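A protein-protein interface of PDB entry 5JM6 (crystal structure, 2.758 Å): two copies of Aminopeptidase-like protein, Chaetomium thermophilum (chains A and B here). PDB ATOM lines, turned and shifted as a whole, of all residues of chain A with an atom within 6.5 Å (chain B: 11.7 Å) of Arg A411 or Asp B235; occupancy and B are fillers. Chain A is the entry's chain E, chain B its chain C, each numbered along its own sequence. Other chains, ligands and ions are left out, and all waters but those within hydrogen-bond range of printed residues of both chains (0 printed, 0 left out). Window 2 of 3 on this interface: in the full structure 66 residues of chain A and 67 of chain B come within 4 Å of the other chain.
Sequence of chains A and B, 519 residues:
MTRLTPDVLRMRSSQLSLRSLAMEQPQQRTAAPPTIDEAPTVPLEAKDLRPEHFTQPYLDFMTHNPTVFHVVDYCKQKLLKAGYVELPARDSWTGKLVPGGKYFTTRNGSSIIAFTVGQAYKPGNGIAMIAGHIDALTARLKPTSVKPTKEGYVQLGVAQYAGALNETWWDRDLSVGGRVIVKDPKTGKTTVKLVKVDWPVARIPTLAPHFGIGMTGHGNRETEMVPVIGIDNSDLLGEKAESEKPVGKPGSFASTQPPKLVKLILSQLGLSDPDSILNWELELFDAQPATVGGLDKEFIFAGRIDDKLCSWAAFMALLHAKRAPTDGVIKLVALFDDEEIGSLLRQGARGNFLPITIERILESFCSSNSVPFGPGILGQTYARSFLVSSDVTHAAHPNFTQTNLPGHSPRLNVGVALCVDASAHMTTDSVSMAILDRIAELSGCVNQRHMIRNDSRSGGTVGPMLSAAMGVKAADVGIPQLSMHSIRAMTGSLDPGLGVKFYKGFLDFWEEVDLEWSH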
ATOM      1  N   ALA A 395      -9.791 -27.363 -17.291  1.00  0.00           N
ATOM      2  CA  ALA A 395     -10.674 -27.031 -18.396  1.00  0.00           C
ATOM      3  C   ALA A 395     -11.971 -26.466 -17.834  1.00  0.00           C
ATOM      4  O   ALA A 395     -12.270 -26.644 -16.651  1.00  0.00           O
ATOM      5  CB  ALA A 395     -10.944 -28.250 -19.260  1.00  0.00           C
ATOM      6  N   ALA A 396     -12.721 -25.760 -18.672  1.00  0.00           N
ATOM      7  CA  ALA A 396     -14.042 -25.281 -18.284  1.00  0.00           C
ATOM      8  C   ALA A 396     -14.899 -26.459 -17.842  1.00  0.00           C
ATOM      9  O   ALA A 396     -15.000 -27.455 -18.554  1.00  0.00           O
ATOM     10  CB  ALA A 396     -14.703 -24.543 -19.437  1.00  0.00           C
ATOM     11  N   SER A 409     -11.217 -19.676 -19.067  1.00  0.00           N
ATOM     12  CA  SER A 409     -11.556 -21.090 -18.833  1.00  0.00           C
ATOM     13  C   SER A 409     -11.403 -21.958 -20.092  1.00  0.00           C
ATOM     14  O   SER A 409     -12.296 -21.991 -20.938  1.00  0.00           O
ATOM     15  CB  SER A 409     -12.984 -21.212 -18.300  1.00  0.00           C
ATOM     16  OG  SER A 409     -13.126 -20.529 -17.068  1.00  0.00           O
ATOM     17  N   PRO A 410     -10.252 -22.641 -20.230  1.00  0.00           N
ATOM     18  CA  PRO A 410      -9.841 -23.317 -21.471  1.00  0.00           C
ATOM     19  C   PRO A 410     -10.696 -24.513 -21.912  1.00  0.00           C
ATOM     20  O   PRO A 410     -11.184 -25.301 -21.100  1.00  0.00           O
ATOM     21  CB  PRO A 410      -8.415 -23.789 -21.157  1.00  0.00           C
ATOM     22  CG  PRO A 410      -8.003 -23.033 -19.930  1.00  0.00           C
ATOM     23  CD  PRO A 410      -9.258 -22.827 -19.161  1.00  0.00           C
ATOM     24  N   ARG A 411     -10.872 -24.601 -23.227  1.00  0.00           N
ATOM     25  CA  ARG A 411     -11.587 -25.676 -23.913  1.00  0.00           C
ATOM     26  C   ARG A 411     -10.740 -26.919 -24.185  1.00  0.00           C
ATOM     27  O   ARG A 411      -9.512 -26.845 -24.232  1.00  0.00           O
ATOM     28  CB  ARG A 411     -12.140 -25.146 -25.230  1.00  0.00           C
ATOM     29  CG  ARG A 411     -12.841 -23.818 -25.077  1.00  0.00           C
ATOM     30  CD  ARG A 411     -14.211 -24.008 -24.470  1.00  0.00           C
ATOM     31  NE  ARG A 411     -15.257 -23.758 -25.453  1.00  0.00           N
ATOM     32  CZ  ARG A 411     -16.069 -22.708 -25.422  1.00  0.00           C
ATOM     33  NH1 ARG A 411     -15.966 -21.819 -24.443  1.00  0.00           N
ATOM     34  NH2 ARG A 411     -16.991 -22.552 -26.361  1.00  0.00           N
ATOM     35  N   LEU A 412     -11.397 -28.059 -24.363  1.00  0.00           N
ATOM     36  CA  LEU A 412     -10.705 -29.258 -24.825  1.00  0.00           C
ATOM     37  C   LEU A 412     -10.493 -29.235 -26.340  1.00  0.00           C
ATOM     38  O   LEU A 412     -11.277 -28.634 -27.076  1.00  0.00           O
ATOM     39  CB  LEU A 412     -11.474 -30.515 -24.426  1.00  0.00           C
ATOM     40  CG  LEU A 412     -11.697 -30.733 -22.931  1.00  0.00           C
ATOM     41  CD1 LEU A 412     -12.303 -32.106 -22.681  1.00  0.00           C
ATOM     42  CD2 LEU A 412     -10.391 -30.566 -22.174  1.00  0.00           C
ATOM     43  N   ASN A 413      -9.428 -29.897 -26.786  1.00  0.00           N
ATOM     44  CA  ASN A 413      -9.079 -30.001 -28.205  1.00  0.00           C
ATOM     45  C   ASN A 413      -8.910 -28.651 -28.896  1.00  0.00           C
ATOM     46  O   ASN A 413      -9.426 -28.431 -29.990  1.00  0.00           O
ATOM     47  CB  ASN A 413     -10.127 -30.829 -28.952  1.00  0.00           C
ATOM     48  CG  ASN A 413     -10.038 -32.306 -28.631  1.00  0.00           C
ATOM     49  OD1 ASN A 413      -9.004 -32.791 -28.172  1.00  0.00           O
ATOM     50  ND2 ASN A 413     -11.124 -33.030 -28.872  1.00  0.00           N
ATOM     51  N   VAL A 414      -8.184 -27.749 -28.249  1.00  0.00           N
ATOM     52  CA  VAL A 414      -7.897 -26.440 -28.823  1.00  0.00           C
ATOM     53  C   VAL A 414      -6.402 -26.168 -28.759  1.00  0.00           C
ATOM     54  O   VAL A 414      -5.763 -25.886 -29.772  1.00  0.00           O
ATOM     55  CB  VAL A 414      -8.693 -25.325 -28.126  1.00  0.00           C
ATOM     56  CG1 VAL A 414      -8.074 -23.970 -28.405  1.00  0.00           C
ATOM     57  CG2 VAL A 414     -10.133 -25.353 -28.608  1.00  0.00           C
ATOM     58  N   GLY A 415      -5.855 -26.197 -27.554  1.00  0.00           N
ATOM     59  CA  GLY A 415      -4.432 -26.012 -27.387  1.00  0.00           C
ATOM     60  C   GLY A 415      -4.094 -25.709 -25.952  1.00  0.00           C
ATOM     61  O   GLY A 415      -4.967 -25.655 -25.085  1.00  0.00           O
ATOM     62  N   GLN A 448      -4.489 -20.734 -25.147  1.00  0.00           N
ATOM     63  CA  GLN A 448      -5.615 -20.332 -24.321  1.00  0.00           C
ATOM     64  C   GLN A 448      -5.100 -19.644 -23.059  1.00  0.00           C
ATOM     65  O   GLN A 448      -3.891 -19.560 -22.840  1.00  0.00           O
ATOM     66  CB  GLN A 448      -6.481 -21.548 -23.979  1.00  0.00           C
ATOM     67  CG  GLN A 448      -6.854 -22.383 -25.198  1.00  0.00           C
ATOM     68  CD  GLN A 448      -7.919 -23.421 -24.905  1.00  0.00           C
ATOM     69  OE1 GLN A 448      -9.077 -23.086 -24.659  1.00  0.00           O
ATOM     70  NE2 GLN A 448      -7.531 -24.691 -24.933  1.00  0.00           N
ATOM     71  N   PRO A 480      -5.267 -28.379 -20.808  1.00  0.00           N
ATOM     72  CA  PRO A 480      -6.495 -28.390 -20.009  1.00  0.00           C
ATOM     73  C   PRO A 480      -6.997 -29.799 -19.720  1.00  0.00           C
ATOM     74  O   PRO A 480      -6.784 -30.729 -20.501  1.00  0.00           O
ATOM     75  CB  PRO A 480      -7.490 -27.613 -20.875  1.00  0.00           C
ATOM     76  CG  PRO A 480      -6.971 -27.740 -22.258  1.00  0.00           C
ATOM     77  CD  PRO A 480      -5.475 -27.779 -22.137  1.00  0.00           C
ATOM     78  N   ASP A 495      -5.508 -33.330 -27.309  1.00  0.00           N
ATOM     79  CA  ASP A 495      -4.738 -32.515 -26.377  1.00  0.00           C
ATOM     80  C   ASP A 495      -3.288 -32.991 -26.159  1.00  0.00           C
ATOM     81  O   ASP A 495      -2.399 -32.155 -26.009  1.00  0.00           O
ATOM     82  CB  ASP A 495      -5.487 -32.401 -25.049  1.00  0.00           C
ATOM     83  CG  ASP A 495      -6.495 -31.259 -25.056  1.00  0.00           C
ATOM     84  OD1 ASP A 495      -6.083 -30.107 -25.315  1.00  0.00           O
ATOM     85  OD2 ASP A 495      -7.696 -31.511 -24.827  1.00  0.00           O
ATOM     86  N   PRO B 148     -28.472 -27.818 -24.277  1.00  0.00           N
ATOM     87  CA  PRO B 148     -27.664 -26.787 -24.936  1.00  0.00           C
ATOM     88  C   PRO B 148     -26.179 -27.095 -24.793  1.00  0.00           C
ATOM     89  O   PRO B 148     -25.754 -27.497 -23.709  1.00  0.00           O
ATOM     90  CB  PRO B 148     -28.027 -25.500 -24.181  1.00  0.00           C
ATOM     91  CG  PRO B 148     -29.197 -25.849 -23.308  1.00  0.00           C
ATOM     92  CD  PRO B 148     -29.118 -27.313 -23.055  1.00  0.00           C
ATOM     93  N   THR B 149     -25.406 -26.923 -25.859  1.00  0.00           N
ATOM     94  CA  THR B 149     -23.962 -27.062 -25.738  1.00  0.00           C
ATOM     95  C   THR B 149     -23.456 -25.951 -24.823  1.00  0.00           C
ATOM     96  O   THR B 149     -23.772 -24.776 -25.017  1.00  0.00           O
ATOM     97  CB  THR B 149     -23.252 -27.013 -27.104  1.00  0.00           C
ATOM     98  OG1 THR B 149     -23.436 -25.724 -27.700  1.00  0.00           O
ATOM     99  CG2 THR B 149     -23.805 -28.090 -28.031  1.00  0.00           C
ATOM    100  N   LYS B 150     -22.681 -26.342 -23.818  1.00  0.00           N
ATOM    101  CA  LYS B 150     -22.349 -25.474 -22.695  1.00  0.00           C
ATOM    102  C   LYS B 150     -20.845 -25.494 -22.441  1.00  0.00           C
ATOM    103  O   LYS B 150     -20.278 -26.547 -22.142  1.00  0.00           O
ATOM    104  CB  LYS B 150     -23.125 -25.936 -21.461  1.00  0.00           C
ATOM    105  CG  LYS B 150     -23.080 -25.055 -20.228  1.00  0.00           C
ATOM    106  CD  LYS B 150     -24.050 -25.650 -19.214  1.00  0.00           C
ATOM    107  CE  LYS B 150     -24.517 -24.666 -18.164  1.00  0.00           C
ATOM    108  NZ  LYS B 150     -25.513 -25.327 -17.270  1.00  0.00           N
ATOM    109  N   GLU B 151     -20.212 -24.330 -22.570  1.00  0.00           N
ATOM    110  CA  GLU B 151     -18.756 -24.187 -22.491  1.00  0.00           C
ATOM    111  C   GLU B 151     -18.045 -25.155 -23.443  1.00  0.00           C
ATOM    112  O   GLU B 151     -16.974 -25.675 -23.132  1.00  0.00           O
ATOM    113  CB  GLU B 151     -18.258 -24.394 -21.053  1.00  0.00           C
ATOM    114  CG  GLU B 151     -18.963 -23.546 -19.983  1.00  0.00           C
ATOM    115  CD  GLU B 151     -18.444 -22.113 -19.878  1.00  0.00           C
ATOM    116  OE1 GLU B 151     -18.815 -21.422 -18.904  1.00  0.00           O
ATOM    117  OE2 GLU B 151     -17.669 -21.677 -20.757  1.00  0.00           O
ATOM    118  N   GLY B 152     -18.653 -25.396 -24.602  1.00  0.00           N
ATOM    119  CA  GLY B 152     -18.045 -26.226 -25.628  1.00  0.00           C
ATOM    120  C   GLY B 152     -18.367 -27.707 -25.531  1.00  0.00           C
ATOM    121  O   GLY B 152     -17.991 -28.485 -26.409  1.00  0.00           O
ATOM    122  N   TYR B 153     -19.063 -28.099 -24.469  1.00  0.00           N
ATOM    123  CA  TYR B 153     -19.410 -29.501 -24.257  1.00  0.00           C
ATOM    124  C   TYR B 153     -20.820 -29.818 -24.734  1.00  0.00           C
ATOM    125  O   TYR B 153     -21.739 -29.018 -24.565  1.00  0.00           O
ATOM    126  CB  TYR B 153     -19.289 -29.873 -22.778  1.00  0.00           C
ATOM    127  CG  TYR B 153     -17.909 -29.703 -22.192  1.00  0.00           C
ATOM    128  CD1 TYR B 153     -17.477 -28.467 -21.735  1.00  0.00           C
ATOM    129  CD2 TYR B 153     -17.045 -30.784 -22.078  1.00  0.00           C
ATOM    130  CE1 TYR B 153     -16.221 -28.308 -21.191  1.00  0.00           C
ATOM    131  CE2 TYR B 153     -15.785 -30.635 -21.533  1.00  0.00           C
ATOM    132  CZ  TYR B 153     -15.378 -29.395 -21.091  1.00  0.00           C
ATOM    133  OH  TYR B 153     -14.123 -29.244 -20.548  1.00  0.00           O
ATOM    134  N   VAL B 154     -20.979 -30.998 -25.323  1.00  0.00           N
ATOM    135  CA  VAL B 154     -22.291 -31.533 -25.659  1.00  0.00           C
ATOM    136  C   VAL B 154     -22.747 -32.433 -24.519  1.00  0.00           C
ATOM    137  O   VAL B 154     -22.027 -33.349 -24.123  1.00  0.00           O
ATOM    138  CB  VAL B 154     -22.260 -32.325 -26.977  1.00  0.00           C
ATOM    139  CG1 VAL B 154     -23.664 -32.756 -27.377  1.00  0.00           C
ATOM    140  CG2 VAL B 154     -21.620 -31.491 -28.074  1.00  0.00           C
ATOM    141  N   VAL B 228     -21.596 -35.788 -19.964  1.00  0.00           N
ATOM    142  CA  VAL B 228     -20.941 -35.128 -21.084  1.00  0.00           C
ATOM    143  C   VAL B 228     -20.669 -36.145 -22.193  1.00  0.00           C
ATOM    144  O   VAL B 228     -20.009 -37.159 -21.963  1.00  0.00           O
ATOM    145  CB  VAL B 228     -19.632 -34.458 -20.627  1.00  0.00           C
ATOM    146  CG1 VAL B 228     -18.690 -34.276 -21.786  1.00  0.00           C
ATOM    147  CG2 VAL B 228     -19.930 -33.126 -19.959  1.00  0.00           C
ATOM    148  N   GLY B 230     -19.689 -35.202 -25.613  1.00  0.00           N
ATOM    149  CA  GLY B 230     -18.870 -34.733 -26.717  1.00  0.00           C
ATOM    150  C   GLY B 230     -18.455 -33.278 -26.638  1.00  0.00           C
ATOM    151  O   GLY B 230     -18.828 -32.557 -25.713  1.00  0.00           O
ATOM    152  N   ILE B 231     -17.677 -32.854 -27.630  1.00  0.00           N
ATOM    153  CA  ILE B 231     -17.153 -31.497 -27.708  1.00  0.00           C
ATOM    154  C   ILE B 231     -17.696 -30.792 -28.946  1.00  0.00           C
ATOM    155  O   ILE B 231     -17.772 -31.397 -30.015  1.00  0.00           O
ATOM    156  CB  ILE B 231     -15.609 -31.501 -27.764  1.00  0.00           C
ATOM    157  CG1 ILE B 231     -15.021 -32.062 -26.473  1.00  0.00           C
ATOM    158  CG2 ILE B 231     -15.063 -30.107 -28.026  1.00  0.00           C
ATOM    159  CD1 ILE B 231     -13.536 -32.268 -26.552  1.00  0.00           C
ATOM    160  N   ASP B 232     -18.149 -29.551 -28.791  1.00  0.00           N
ATOM    161  CA  ASP B 232     -18.340 -28.671 -29.941  1.00  0.00           C
ATOM    162  C   ASP B 232     -17.859 -27.257 -29.610  1.00  0.00           C
ATOM    163  O   ASP B 232     -18.497 -26.543 -28.837  1.00  0.00           O
ATOM    164  CB  ASP B 232     -19.812 -28.670 -30.360  1.00  0.00           C
ATOM    165  CG  ASP B 232     -20.070 -27.839 -31.604  1.00  0.00           C
ATOM    166  OD1 ASP B 232     -20.286 -28.433 -32.682  1.00  0.00           O
ATOM    167  OD2 ASP B 232     -20.075 -26.594 -31.502  1.00  0.00           O
ATOM    168  N   ASN B 233     -16.754 -26.852 -30.227  1.00  0.00           N
ATOM    169  CA  ASN B 233     -16.129 -25.549 -29.992  1.00  0.00           C
ATOM    170  C   ASN B 233     -16.453 -24.491 -31.048  1.00  0.00           C
ATOM    171  O   ASN B 233     -15.800 -23.449 -31.105  1.00  0.00           O
ATOM    172  CB  ASN B 233     -14.616 -25.709 -29.854  1.00  0.00           C
ATOM    173  CG  ASN B 233     -14.212 -26.260 -28.496  1.00  0.00           C
ATOM    174  OD1 ASN B 233     -14.772 -25.881 -27.465  1.00  0.00           O
ATOM    175  ND2 ASN B 233     -13.239 -27.161 -28.491  1.00  0.00           N
ATOM    176  N   SER B 234     -17.417 -24.782 -31.915  1.00  0.00           N
ATOM    177  CA  SER B 234     -17.663 -23.982 -33.118  1.00  0.00           C
ATOM    178  C   SER B 234     -18.061 -22.520 -32.865  1.00  0.00           C
ATOM    179  O   SER B 234     -18.213 -21.747 -33.809  1.00  0.00           O
ATOM    180  CB  SER B 234     -18.734 -24.659 -33.979  1.00  0.00           C
ATOM    181  OG  SER B 234     -19.863 -25.029 -33.210  1.00  0.00           O
ATOM    182  N   ASP B 235     -18.228 -22.143 -31.601  1.00  0.00           N
ATOM    183  CA  ASP B 235     -18.541 -20.761 -31.234  1.00  0.00           C
ATOM    184  C   ASP B 235     -17.268 -19.922 -31.066  1.00  0.00           C
ATOM    185  O   ASP B 235     -17.301 -18.854 -30.458  1.00  0.00           O
ATOM    186  CB  ASP B 235     -19.390 -20.701 -29.960  1.00  0.00           C
ATOM    187  CG  ASP B 235     -18.731 -21.382 -28.780  1.00  0.00           C
ATOM    188  OD1 ASP B 235     -18.046 -22.404 -28.988  1.00  0.00           O
ATOM    189  OD2 ASP B 235     -18.904 -20.897 -27.641  1.00  0.00           O
ATOM    190  N   LEU B 236     -16.137 -20.449 -31.524  1.00  0.00           N
ATOM    191  CA  LEU B 236     -14.862 -19.748 -31.391  1.00  0.00           C
ATOM    192  C   LEU B 236     -14.274 -19.301 -32.732  1.00  0.00           C
ATOM    193  O   LEU B 236     -13.527 -18.321 -32.799  1.00  0.00           O
ATOM    194  CB  LEU B 236     -13.864 -20.640 -30.661  1.00  0.00           C
ATOM    195  CG  LEU B 236     -14.310 -21.186 -29.304  1.00  0.00           C
ATOM    196  CD1 LEU B 236     -13.521 -22.436 -28.981  1.00  0.00           C
ATOM    197  CD2 LEU B 236     -14.130 -20.154 -28.203  1.00  0.00           C
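The side-chain carboxylate (OD1) of Asp B235 is in salt-bridge range of the guanidinium group (NH2) of Arg A411 (2.8 Å). The backbone carbonyl oxygen (O) of Leu A412 sits at hydrogen-bond distance from the side-chain amide nitrogen (ND2) of Asn B233. The backbone carbonyl oxygen of Ala A396 sits at hydrogen-bond distance from the side-chain hydroxyl of Tyr B153 (2.8 Å). The guanidinium group (NE) of Arg A411 is in hydrogen-bond range of the side-chain amide oxygen (OD1) of Asn B233 (3.0 Å). NE of Arg A411 lies within hydrogen-bond range of O of Glu B151, at 3.5 Å.
O of Gly B152 is in hydrogen-bond range of N of Asp B232. N of Arg A411 lies within hydrogen-bond range of OE1 of Gln A448 (2.8 Å). The backbone carbonyl oxygen (O) of Pro A410 is in hydrogen-bond range of the backbone NH (N) of Ala A396, 2.9 Å away. The side-chain carboxylate of Asp A495 lies within hydrogen-bond range of the backbone NH of Asn A413 (3.1 Å).
CB of Ala A395 touches OH of Tyr B153, 3.6 Å away. Glu B151 touches Ala A396. NE of Arg A411 touches CA of Gly B152, at 3.7 Å. OH of Tyr B153 touches CG of Leu A412, 3.7 Å away. Leu A412 touches Ile B231. Asn A413 touches Ile B231 (ND2 to CD1, 3.4 Å). Val A414 touches Asn B233 (CG2 to ND2, 3.6 Å).
Of chain B, only Tyr B153 comes within 4 Å of Ala A395. Of chain B, only Glu B151 and Tyr B153 come within 4 Å of Ala A396. Arg A411 touches four residues of chain B. Of the printed residues of chain B, Asn A413 touches Ile B231 (3.4 Å). Val A414 touches just one residue of chain B: Asn B233. No residue of chain B comes within 4 Å of Gly A415. No residue of chain B comes within 4 Å of Pro A480. Of the printed residues of chain A, Glu B151 touches Ala A396 and Arg A411. Val B228 touches none of the printed residues of chain A. Printed residues of chain A within 4 Å of Asn B233: Arg A411, Leu A412 and Val A414. Asp B235 touches just one residue of chain A: Arg A411. The nearest residue of chain B that does not touch Arg A411 is Leu B236 (4.1 Å). The nearest printed residue of chain A that does not touch Asp B235 is Val A414 (8.5 Å).
Of the 15 printed residues of chain B, 6 touch a printed residue of chain A. Hydrophobic or aromatic side chains of chain A within 4 Å of the printed part of chain B: Ala A395, Ala A396, Leu A412 and Val A414. Among the printed residues, Asp or Glu carboxylates within 4 Å of a Lys or Arg side-chain nitrogen of the other chain: Arg A411 with Asp B235.
No position is printed for both chains. Of the 12 pairs that touch across the chains among the printed residues, none has its exchanged pair printed and touching as well.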
